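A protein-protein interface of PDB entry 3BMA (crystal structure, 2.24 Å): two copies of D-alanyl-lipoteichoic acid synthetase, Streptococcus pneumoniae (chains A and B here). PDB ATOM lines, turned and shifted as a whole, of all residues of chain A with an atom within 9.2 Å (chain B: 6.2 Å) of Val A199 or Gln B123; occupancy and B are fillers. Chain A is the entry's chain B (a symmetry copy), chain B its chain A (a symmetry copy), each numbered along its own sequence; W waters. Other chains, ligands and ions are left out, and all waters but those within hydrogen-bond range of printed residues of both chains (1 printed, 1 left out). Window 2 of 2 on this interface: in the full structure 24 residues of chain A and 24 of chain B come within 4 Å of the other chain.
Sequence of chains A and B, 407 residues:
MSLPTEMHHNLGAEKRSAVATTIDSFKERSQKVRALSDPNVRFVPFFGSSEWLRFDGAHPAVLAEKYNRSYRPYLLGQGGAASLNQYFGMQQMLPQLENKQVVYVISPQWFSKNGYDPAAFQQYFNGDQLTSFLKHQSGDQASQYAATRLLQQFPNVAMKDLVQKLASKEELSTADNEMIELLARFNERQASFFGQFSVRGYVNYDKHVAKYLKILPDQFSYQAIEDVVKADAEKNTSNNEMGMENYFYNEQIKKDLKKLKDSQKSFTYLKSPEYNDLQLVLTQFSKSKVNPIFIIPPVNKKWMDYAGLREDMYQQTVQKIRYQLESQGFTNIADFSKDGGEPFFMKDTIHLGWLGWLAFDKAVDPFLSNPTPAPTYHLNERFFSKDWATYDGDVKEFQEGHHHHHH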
ATOM      1  N   ALA A  13      23.056  22.458  32.623  1.00  0.00           N
ATOM      2  CA  ALA A  13      22.650  21.695  31.441  1.00  0.00           C
ATOM      3  C   ALA A  13      22.612  20.203  31.727  1.00  0.00           C
ATOM      4  O   ALA A  13      21.773  19.483  31.187  1.00  0.00           O
ATOM      5  CB  ALA A  13      23.579  21.984  30.272  1.00  0.00           C
ATOM      6  N   ARG A  16      19.509  19.475  33.859  1.00  0.00           N
ATOM      7  CA  ARG A  16      18.376  19.430  32.928  1.00  0.00           C
ATOM      8  C   ARG A  16      18.341  18.147  32.095  1.00  0.00           C
ATOM      9  O   ARG A  16      17.272  17.574  31.902  1.00  0.00           O
ATOM     10  CB  ARG A  16      18.359  20.658  32.015  1.00  0.00           C
ATOM     11  CG  ARG A  16      17.998  21.942  32.728  1.00  0.00           C
ATOM     12  CD  ARG A  16      18.043  23.136  31.800  1.00  0.00           C
ATOM     13  NE  ARG A  16      18.872  24.205  32.356  1.00  0.00           N
ATOM     14  CZ  ARG A  16      19.991  24.661  31.797  1.00  0.00           C
ATOM     15  NH1 ARG A  16      20.417  24.167  30.642  1.00  0.00           N
ATOM     16  NH2 ARG A  16      20.680  25.630  32.386  1.00  0.00           N
ATOM     17  N   SER A  17      19.505  17.701  31.625  1.00  0.00           N
ATOM     18  CA  SER A  17      19.629  16.467  30.837  1.00  0.00           C
ATOM     19  C   SER A  17      19.239  15.233  31.642  1.00  0.00           C
ATOM     20  O   SER A  17      18.598  14.325  31.116  1.00  0.00           O
ATOM     21  CB  SER A  17      21.061  16.275  30.332  1.00  0.00           C
ATOM     22  OG  SER A  17      21.487  17.366  29.538  1.00  0.00           O
ATOM     23  N   ALA A  20      15.472  15.095  31.936  1.00  0.00           N
ATOM     24  CA  ALA A  20      14.796  15.352  30.656  1.00  0.00           C
ATOM     25  C   ALA A  20      13.846  14.224  30.271  1.00  0.00           C
ATOM     26  O   ALA A  20      12.746  14.482  29.766  1.00  0.00           O
ATOM     27  CB  ALA A  20      15.817  15.592  29.541  1.00  0.00           C
ATOM     28  N   THR A  22      13.861  11.988  27.905  1.00  0.00           N
ATOM     29  CA  THR A  22      13.538  12.042  26.483  1.00  0.00           C
ATOM     30  C   THR A  22      14.241  10.900  25.748  1.00  0.00           C
ATOM     31  O   THR A  22      15.059  10.187  26.343  1.00  0.00           O
ATOM     32  CB  THR A  22      13.981  13.385  25.866  1.00  0.00           C
ATOM     33  OG1 THR A  22      15.351  13.631  26.192  1.00  0.00           O
ATOM     34  CG2 THR A  22      13.131  14.545  26.388  1.00  0.00           C
ATOM     35  N   ASP A  24      16.287  11.462  23.242  1.00  0.00           N
ATOM     36  CA  ASP A  24      17.628  12.031  23.130  1.00  0.00           C
ATOM     37  C   ASP A  24      18.507  11.812  24.360  1.00  0.00           C
ATOM     38  O   ASP A  24      19.675  11.463  24.222  1.00  0.00           O
ATOM     39  CB  ASP A  24      17.551  13.526  22.804  1.00  0.00           C
ATOM     40  CG  ASP A  24      17.701  13.808  21.318  1.00  0.00           C
ATOM     41  OD1 ASP A  24      18.175  14.913  20.970  1.00  0.00           O
ATOM     42  OD2 ASP A  24      17.356  12.925  20.499  1.00  0.00           O
ATOM     43  N   SER A  25      17.952  12.011  25.554  1.00  0.00           N
ATOM     44  CA  SER A  25      18.700  11.777  26.795  1.00  0.00           C
ATOM     45  C   SER A  25      19.107  10.311  26.943  1.00  0.00           C
ATOM     46  O   SER A  25      20.160  10.007  27.499  1.00  0.00           O
ATOM     47  CB  SER A  25      17.902  12.237  28.014  1.00  0.00           C
ATOM     48  OG  SER A  25      16.807  11.374  28.269  1.00  0.00           O
ATOM     49  N   GLN A  31      24.788  13.825  25.914  1.00  0.00           N
ATOM     50  CA  GLN A  31      24.161  14.241  27.171  1.00  0.00           C
ATOM     51  C   GLN A  31      24.508  13.365  28.376  1.00  0.00           C
ATOM     52  O   GLN A  31      24.859  13.888  29.439  1.00  0.00           O
ATOM     53  CB  GLN A  31      22.645  14.364  26.996  1.00  0.00           C
ATOM     54  CG  GLN A  31      22.213  15.365  25.921  1.00  0.00           C
ATOM     55  CD  GLN A  31      20.702  15.504  25.818  1.00  0.00           C
ATOM     56  OE1 GLN A  31      20.131  15.375  24.739  1.00  0.00           O
ATOM     57  NE2 GLN A  31      20.048  15.766  26.946  1.00  0.00           N
ATOM     58  N   ARG A  34      28.444  13.428  29.160  1.00  0.00           N
ATOM     59  CA  ARG A  34      28.788  14.714  29.776  1.00  0.00           C
ATOM     60  C   ARG A  34      28.531  14.711  31.283  1.00  0.00           C
ATOM     61  O   ARG A  34      29.386  15.127  32.068  1.00  0.00           O
ATOM     62  CB  ARG A  34      28.003  15.857  29.121  1.00  0.00           C
ATOM     63  CG  ARG A  34      28.604  17.243  29.337  1.00  0.00           C
ATOM     64  CD  ARG A  34      27.670  18.366  28.886  1.00  0.00           C
ATOM     65  NE  ARG A  34      27.141  18.156  27.536  1.00  0.00           N
ATOM     66  CZ  ARG A  34      25.848  18.152  27.222  1.00  0.00           C
ATOM     67  NH1 ARG A  34      24.925  18.366  28.152  1.00  0.00           N
ATOM     68  NH2 ARG A  34      25.475  17.947  25.966  1.00  0.00           N
ATOM     69  N   PHE A 194      28.005  17.598  17.733  1.00  0.00           N
ATOM     70  CA  PHE A 194      26.708  18.180  17.372  1.00  0.00           C
ATOM     71  C   PHE A 194      25.617  17.977  18.424  1.00  0.00           C
ATOM     72  O   PHE A 194      24.697  18.792  18.528  1.00  0.00           O
ATOM     73  CB  PHE A 194      26.241  17.684  15.999  1.00  0.00           C
ATOM     74  CG  PHE A 194      27.134  18.111  14.866  1.00  0.00           C
ATOM     75  CD1 PHE A 194      27.973  17.193  14.242  1.00  0.00           C
ATOM     76  CD2 PHE A 194      27.147  19.434  14.432  1.00  0.00           C
ATOM     77  CE1 PHE A 194      28.811  17.585  13.196  1.00  0.00           C
ATOM     78  CE2 PHE A 194      27.980  19.837  13.387  1.00  0.00           C
ATOM     79  CZ  PHE A 194      28.813  18.913  12.768  1.00  0.00           C
ATOM     80  N   GLY A 195      25.732  16.901  19.203  1.00  0.00           N
ATOM     81  CA  GLY A 195      24.753  16.569  20.241  1.00  0.00           C
ATOM     82  C   GLY A 195      24.765  17.481  21.456  1.00  0.00           C
ATOM     83  O   GLY A 195      23.806  17.493  22.236  1.00  0.00           O
ATOM     84  N   GLN A 196      25.845  18.248  21.615  1.00  0.00           N
ATOM     85  CA  GLN A 196      25.982  19.201  22.715  1.00  0.00           C
ATOM     86  C   GLN A 196      25.094  20.445  22.544  1.00  0.00           C
ATOM     87  O   GLN A 196      24.952  21.249  23.468  1.00  0.00           O
ATOM     88  CB  GLN A 196      27.456  19.599  22.902  1.00  0.00           C
ATOM     89  CG  GLN A 196      27.946  20.726  21.992  1.00  0.00           C
ATOM     90  CD  GLN A 196      29.455  20.923  22.034  1.00  0.00           C
ATOM     91  OE1 GLN A 196      30.051  21.040  23.104  1.00  0.00           O
ATOM     92  NE2 GLN A 196      30.076  20.978  20.858  1.00  0.00           N
ATOM     93  N   PHE A 197      24.496  20.592  21.364  1.00  0.00           N
ATOM     94  CA  PHE A 197      23.652  21.746  21.057  1.00  0.00           C
ATOM     95  C   PHE A 197      22.162  21.455  21.224  1.00  0.00           C
ATOM     96  O   PHE A 197      21.331  22.337  21.014  1.00  0.00           O
ATOM     97  CB  PHE A 197      23.943  22.256  19.642  1.00  0.00           C
ATOM     98  CG  PHE A 197      25.397  22.563  19.393  1.00  0.00           C
ATOM     99  CD1 PHE A 197      26.061  23.529  20.148  1.00  0.00           C
ATOM    100  CD2 PHE A 197      26.105  21.888  18.405  1.00  0.00           C
ATOM    101  CE1 PHE A 197      27.404  23.815  19.920  1.00  0.00           C
ATOM    102  CE2 PHE A 197      27.447  22.172  18.173  1.00  0.00           C
ATOM    103  CZ  PHE A 197      28.097  23.134  18.932  1.00  0.00           C
ATOM    104  N   SER A 198      21.838  20.222  21.612  1.00  0.00           N
ATOM    105  CA  SER A 198      20.452  19.784  21.785  1.00  0.00           C
ATOM    106  C   SER A 198      19.839  20.317  23.079  1.00  0.00           C
ATOM    107  O   SER A 198      20.365  20.078  24.168  1.00  0.00           O
ATOM    108  CB  SER A 198      20.367  18.256  21.749  1.00  0.00           C
ATOM    109  OG  SER A 198      19.028  17.808  21.877  1.00  0.00           O
ATOM    110  N   VAL A 199      18.728  21.042  22.940  1.00  0.00           N
ATOM    111  CA  VAL A 199      18.014  21.633  24.077  1.00  0.00           C
ATOM    112  C   VAL A 199      16.640  20.956  24.268  1.00  0.00           C
ATOM    113  O   VAL A 199      15.681  21.581  24.734  1.00  0.00           O
ATOM    114  CB  VAL A 199      17.848  23.187  23.927  1.00  0.00           C
ATOM    115  CG1 VAL A 199      17.955  23.878  25.280  1.00  0.00           C
ATOM    116  CG2 VAL A 199      18.888  23.777  22.977  1.00  0.00           C
ATOM    117  N   ARG A 200      16.563  19.673  23.910  1.00  0.00           N
ATOM    118  CA  ARG A 200      15.319  18.893  23.994  1.00  0.00           C
ATOM    119  C   ARG A 200      14.960  18.502  25.426  1.00  0.00           C
ATOM    120  O   ARG A 200      15.707  17.773  26.087  1.00  0.00           O
ATOM    121  CB  ARG A 200      15.403  17.637  23.120  1.00  0.00           C
ATOM    122  CG  ARG A 200      14.891  17.824  21.705  1.00  0.00           C
ATOM    123  CD  ARG A 200      15.311  16.672  20.815  1.00  0.00           C
ATOM    124  NE  ARG A 200      14.868  16.852  19.435  1.00  0.00           N
ATOM    125  CZ  ARG A 200      15.443  16.288  18.375  1.00  0.00           C
ATOM    126  NH1 ARG A 200      16.507  15.506  18.517  1.00  0.00           N
ATOM    127  NH2 ARG A 200      14.960  16.516  17.164  1.00  0.00           N
ATOM    128  N   GLY A 201      13.808  18.987  25.889  1.00  0.00           N
ATOM    129  CA  GLY A 201      13.316  18.703  27.236  1.00  0.00           C
ATOM    130  C   GLY A 201      14.097  19.412  28.328  1.00  0.00           C
ATOM    131  O   GLY A 201      14.393  18.823  29.372  1.00  0.00           O
ATOM    132  N   TYR A 202      14.426  20.680  28.084  1.00  0.00           N
ATOM    133  CA  TYR A 202      15.201  21.488  29.031  1.00  0.00           C
ATOM    134  C   TYR A 202      14.309  22.403  29.877  1.00  0.00           C
ATOM    135  O   TYR A 202      14.729  22.886  30.932  1.00  0.00           O
ATOM    136  CB  TYR A 202      16.298  22.281  28.300  1.00  0.00           C
ATOM    137  CG  TYR A 202      17.605  21.524  28.104  1.00  0.00           C
ATOM    138  CD1 TYR A 202      17.621  20.222  27.591  1.00  0.00           C
ATOM    139  CD2 TYR A 202      18.830  22.116  28.419  1.00  0.00           C
ATOM    140  CE1 TYR A 202      18.815  19.526  27.414  1.00  0.00           C
ATOM    141  CE2 TYR A 202      20.032  21.430  28.243  1.00  0.00           C
ATOM    142  CZ  TYR A 202      20.015  20.136  27.739  1.00  0.00           C
ATOM    143  OH  TYR A 202      21.194  19.451  27.559  1.00  0.00           O
ATOM    144  N   VAL A 203      13.077  22.623  29.412  1.00  0.00           N
ATOM    145  CA  VAL A 203      12.058  23.350  30.175  1.00  0.00           C
ATOM    146  C   VAL A 203      11.269  22.383  31.078  1.00  0.00           C
ATOM    147  O   VAL A 203      10.512  22.808  31.960  1.00  0.00           O
ATOM    148  CB  VAL A 203      11.124  24.185  29.240  1.00  0.00           C
ATOM    149  CG1 VAL A 203       9.931  23.363  28.737  1.00  0.00           C
ATOM    150  CG2 VAL A 203      10.651  25.457  29.936  1.00  0.00           C
ATOM    151  N   ASN A 204      11.486  21.082  30.865  1.00  0.00           N
ATOM    152  CA  ASN A 204      10.891  20.013  31.674  1.00  0.00           C
ATOM    153  C   ASN A 204      11.385  19.969  33.121  1.00  0.00           C
ATOM    154  O   ASN A 204      10.832  19.241  33.944  1.00  0.00           O
ATOM    155  CB  ASN A 204      11.126  18.647  31.016  1.00  0.00           C
ATOM    156  CG  ASN A 204      10.156  18.361  29.877  1.00  0.00           C
ATOM    157  OD1 ASN A 204       9.057  18.918  29.817  1.00  0.00           O
ATOM    158  ND2 ASN A 204      10.558  17.473  28.974  1.00  0.00           N
ATOM    159  N   ILE B  23      12.133  19.651  14.764  1.00  0.00           N
ATOM    160  CA  ILE B  23      13.551  19.785  14.451  1.00  0.00           C
ATOM    161  C   ILE B  23      13.958  18.620  13.547  1.00  0.00           C
ATOM    162  O   ILE B  23      14.644  18.822  12.548  1.00  0.00           O
ATOM    163  CB  ILE B  23      14.410  19.809  15.745  1.00  0.00           C
ATOM    164  CG1 ILE B  23      14.266  21.163  16.457  1.00  0.00           C
ATOM    165  CG2 ILE B  23      15.875  19.514  15.451  1.00  0.00           C
ATOM    166  CD1 ILE B  23      14.902  21.202  17.836  1.00  0.00           C
ATOM    167  N   LYS B  27      15.802  18.578   9.861  1.00  0.00           N
ATOM    168  CA  LYS B  27      17.246  18.352   9.825  1.00  0.00           C
ATOM    169  C   LYS B  27      17.660  16.947   9.422  1.00  0.00           C
ATOM    170  O   LYS B  27      18.788  16.735   8.978  1.00  0.00           O
ATOM    171  CB  LYS B  27      17.898  18.765  11.156  1.00  0.00           C
ATOM    172  CG  LYS B  27      18.138  17.685  12.199  1.00  0.00           C
ATOM    173  CD  LYS B  27      18.887  18.288  13.392  1.00  0.00           C
ATOM    174  CE  LYS B  27      19.543  17.234  14.266  1.00  0.00           C
ATOM    175  NZ  LYS B  27      18.565  16.422  15.038  1.00  0.00           N
ATOM    176  N   GLY B  79      11.877  27.922  14.179  1.00  0.00           N
ATOM    177  CA  GLY B  79      12.231  29.278  14.600  1.00  0.00           C
ATOM    178  C   GLY B  79      13.731  29.502  14.565  1.00  0.00           C
ATOM    179  O   GLY B  79      14.493  28.740  15.160  1.00  0.00           O
ATOM    180  N   PRO B 118      23.168  32.144  15.811  1.00  0.00           N
ATOM    181  CA  PRO B 118      23.954  30.900  15.799  1.00  0.00           C
ATOM    182  C   PRO B 118      23.457  29.858  16.803  1.00  0.00           C
ATOM    183  O   PRO B 118      23.631  28.660  16.575  1.00  0.00           O
ATOM    184  CB  PRO B 118      25.363  31.368  16.186  1.00  0.00           C
ATOM    185  CG  PRO B 118      25.369  32.846  15.937  1.00  0.00           C
ATOM    186  CD  PRO B 118      23.983  33.282  16.273  1.00  0.00           C
ATOM    187  N   ALA B 119      22.836  30.323  17.889  1.00  0.00           N
ATOM    188  CA  ALA B 119      22.222  29.461  18.907  1.00  0.00           C
ATOM    189  C   ALA B 119      21.015  28.686  18.376  1.00  0.00           C
ATOM    190  O   ALA B 119      20.668  27.629  18.909  1.00  0.00           O
ATOM    191  CB  ALA B 119      21.823  30.288  20.133  1.00  0.00           C
ATOM    192  N   ALA B 120      20.377  29.221  17.335  1.00  0.00           N
ATOM    193  CA  ALA B 120      19.277  28.544  16.655  1.00  0.00           C
ATOM    194  C   ALA B 120      19.792  27.603  15.561  1.00  0.00           C
ATOM    195  O   ALA B 120      19.316  26.481  15.444  1.00  0.00           O
ATOM    196  CB  ALA B 120      18.304  29.561  16.079  1.00  0.00           C
ATOM    197  N   PHE B 121      20.772  28.070  14.786  1.00  0.00           N
ATOM    198  CA  PHE B 121      21.416  27.305  13.699  1.00  0.00           C
ATOM    199  C   PHE B 121      21.901  25.919  14.133  1.00  0.00           C
ATOM    200  O   PHE B 121      21.639  24.920  13.454  1.00  0.00           O
ATOM    201  CB  PHE B 121      22.601  28.109  13.144  1.00  0.00           C
ATOM    202  CG  PHE B 121      23.243  27.506  11.913  1.00  0.00           C
ATOM    203  CD1 PHE B 121      22.862  27.927  10.652  1.00  0.00           C
ATOM    204  CD2 PHE B 121      24.241  26.533  12.019  1.00  0.00           C
ATOM    205  CE1 PHE B 121      23.432  27.373   9.507  1.00  0.00           C
ATOM    206  CE2 PHE B 121      24.827  25.981  10.878  1.00  0.00           C
ATOM    207  CZ  PHE B 121      24.415  26.404   9.617  1.00  0.00           C
ATOM    208  N   GLN B 122      22.610  25.896  15.261  1.00  0.00           N
ATOM    209  CA  GLN B 122      23.200  24.705  15.883  1.00  0.00           C
ATOM    210  C   GLN B 122      22.243  23.538  16.088  1.00  0.00           C
ATOM    211  O   GLN B 122      22.655  22.379  16.084  1.00  0.00           O
ATOM    212  CB  GLN B 122      23.776  25.093  17.248  1.00  0.00           C
ATOM    213  CG  GLN B 122      25.142  25.728  17.180  1.00  0.00           C
ATOM    214  CD  GLN B 122      25.496  26.550  18.406  1.00  0.00           C
ATOM    215  OE1 GLN B 122      26.525  27.229  18.427  1.00  0.00           O
ATOM    216  NE2 GLN B 122      24.654  26.494  19.434  1.00  0.00           N
ATOM    217  N   GLN B 123      20.969  23.858  16.280  1.00  0.00           N
ATOM    218  CA  GLN B 123      19.950  22.864  16.560  1.00  0.00           C
ATOM    219  C   GLN B 123      19.457  22.143  15.313  1.00  0.00           C
ATOM    220  O   GLN B 123      18.869  21.067  15.419  1.00  0.00           O
ATOM    221  CB  GLN B 123      18.767  23.520  17.260  1.00  0.00           C
ATOM    222  CG  GLN B 123      19.102  24.076  18.628  1.00  0.00           C
ATOM    223  CD  GLN B 123      17.902  24.696  19.289  1.00  0.00           C
ATOM    224  OE1 GLN B 123      16.946  24.004  19.640  1.00  0.00           O
ATOM    225  NE2 GLN B 123      17.941  26.010  19.466  1.00  0.00           N
ATOM    226  N   TYR B 124      19.686  22.743  14.144  1.00  0.00           N
ATOM    227  CA  TYR B 124      19.109  22.251  12.883  1.00  0.00           C
ATOM    228  C   TYR B 124      20.170  21.689  11.935  1.00  0.00           C
ATOM    229  O   TYR B 124      19.857  21.208  10.847  1.00  0.00           O
ATOM    230  CB  TYR B 124      18.278  23.349  12.190  1.00  0.00           C
ATOM    231  CG  TYR B 124      17.397  24.149  13.130  1.00  0.00           C
ATOM    232  CD1 TYR B 124      16.612  23.515  14.098  1.00  0.00           C
ATOM    233  CD2 TYR B 124      17.344  25.534  13.046  1.00  0.00           C
ATOM    234  CE1 TYR B 124      15.830  24.238  14.970  1.00  0.00           C
ATOM    235  CE2 TYR B 124      16.540  26.272  13.904  1.00  0.00           C
ATOM    236  CZ  TYR B 124      15.795  25.615  14.869  1.00  0.00           C
ATOM    237  OH  TYR B 124      14.990  26.322  15.729  1.00  0.00           O
ATOM    238  N   PHE B 125      21.422  21.751  12.373  1.00  0.00           N
ATOM    239  CA  PHE B 125      22.551  21.249  11.615  1.00  0.00           C
ATOM    240  C   PHE B 125      23.042  19.951  12.255  1.00  0.00           C
ATOM    241  O   PHE B 125      23.102  19.836  13.482  1.00  0.00           O
ATOM    242  CB  PHE B 125      23.654  22.315  11.582  1.00  0.00           C
ATOM    243  CG  PHE B 125      24.772  22.037  10.602  1.00  0.00           C
ATOM    244  CD1 PHE B 125      24.718  22.526   9.305  1.00  0.00           C
ATOM    245  CD2 PHE B 125      25.897  21.324  10.991  1.00  0.00           C
ATOM    246  CE1 PHE B 125      25.757  22.292   8.412  1.00  0.00           C
ATOM    247  CE2 PHE B 125      26.939  21.085  10.101  1.00  0.00           C
ATOM    248  CZ  PHE B 125      26.862  21.566   8.808  1.00  0.00           C
HETATM  249  O   HOH W   1      17.246  21.420  20.546  1.00  0.00           O
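The side-chain carboxylate (OD1) of Asp A24 is in salt-bridge range of the guanidinium group (NH1) of Arg A200 (3.0 Å).
The backbone carbonyl oxygen of Ala B119 sits at hydrogen-bond distance from the side-chain amide nitrogen of Gln B123.
Phe A194 touches Phe B125 (CE2 to CD2, 3.5 Å).
Phe A197 touches Gln B122.
O of Phe A197 touches CG of Gln B123 (3.7 Å).
Val A199 touches Gln B123 (CG2 to OE1, 3.9 Å).
Ile B23 touches Arg A200.
Val A199 touches one residue of chain B.
Of the printed residues of chain B, Arg A200 touches Ile B23 (3.6 Å).
No residue of chain A comes within 4 Å of Ala B120.
Gln B123 touches just these residues of chain A: Phe A197 (3.7 Å) and Val A199 (3.9 Å).
Printed residues of chain A within 4 Å of Phe B125: Phe A194 (3.5 Å).
The nearest residue of chain B that does not touch Val A199 is Ala B119 (5.9 Å).
Of the 11 printed residues of chain B, 4 touch a printed residue of chain A.
Hydrophobic or aromatic side chains of chain B within 4 Å of the printed part of chain A: Ile B23 and Phe B125.
Of the 20 printed residues of chain A, 4 touch a printed residue of chain B.
Printed residues of chain A that touch a printed residue of chain B: Phe A194, Phe A197, Val A199 and Arg A200.
Hydrophobic or aromatic side chains of chain A within 4 Å of the printed part of chain B: Phe A194, Phe A197 and Val A199.
No position is printed for both chains.
Of the 5 pairs that touch across the chains among the printed residues, none has its exchanged pair printed and touching as well.
Water W1 lies within hydrogen-bond range of the side-chain amide oxygen of Gln B123 (2.8 Å) and the backbone NH of Val A199 (2.8 Å).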
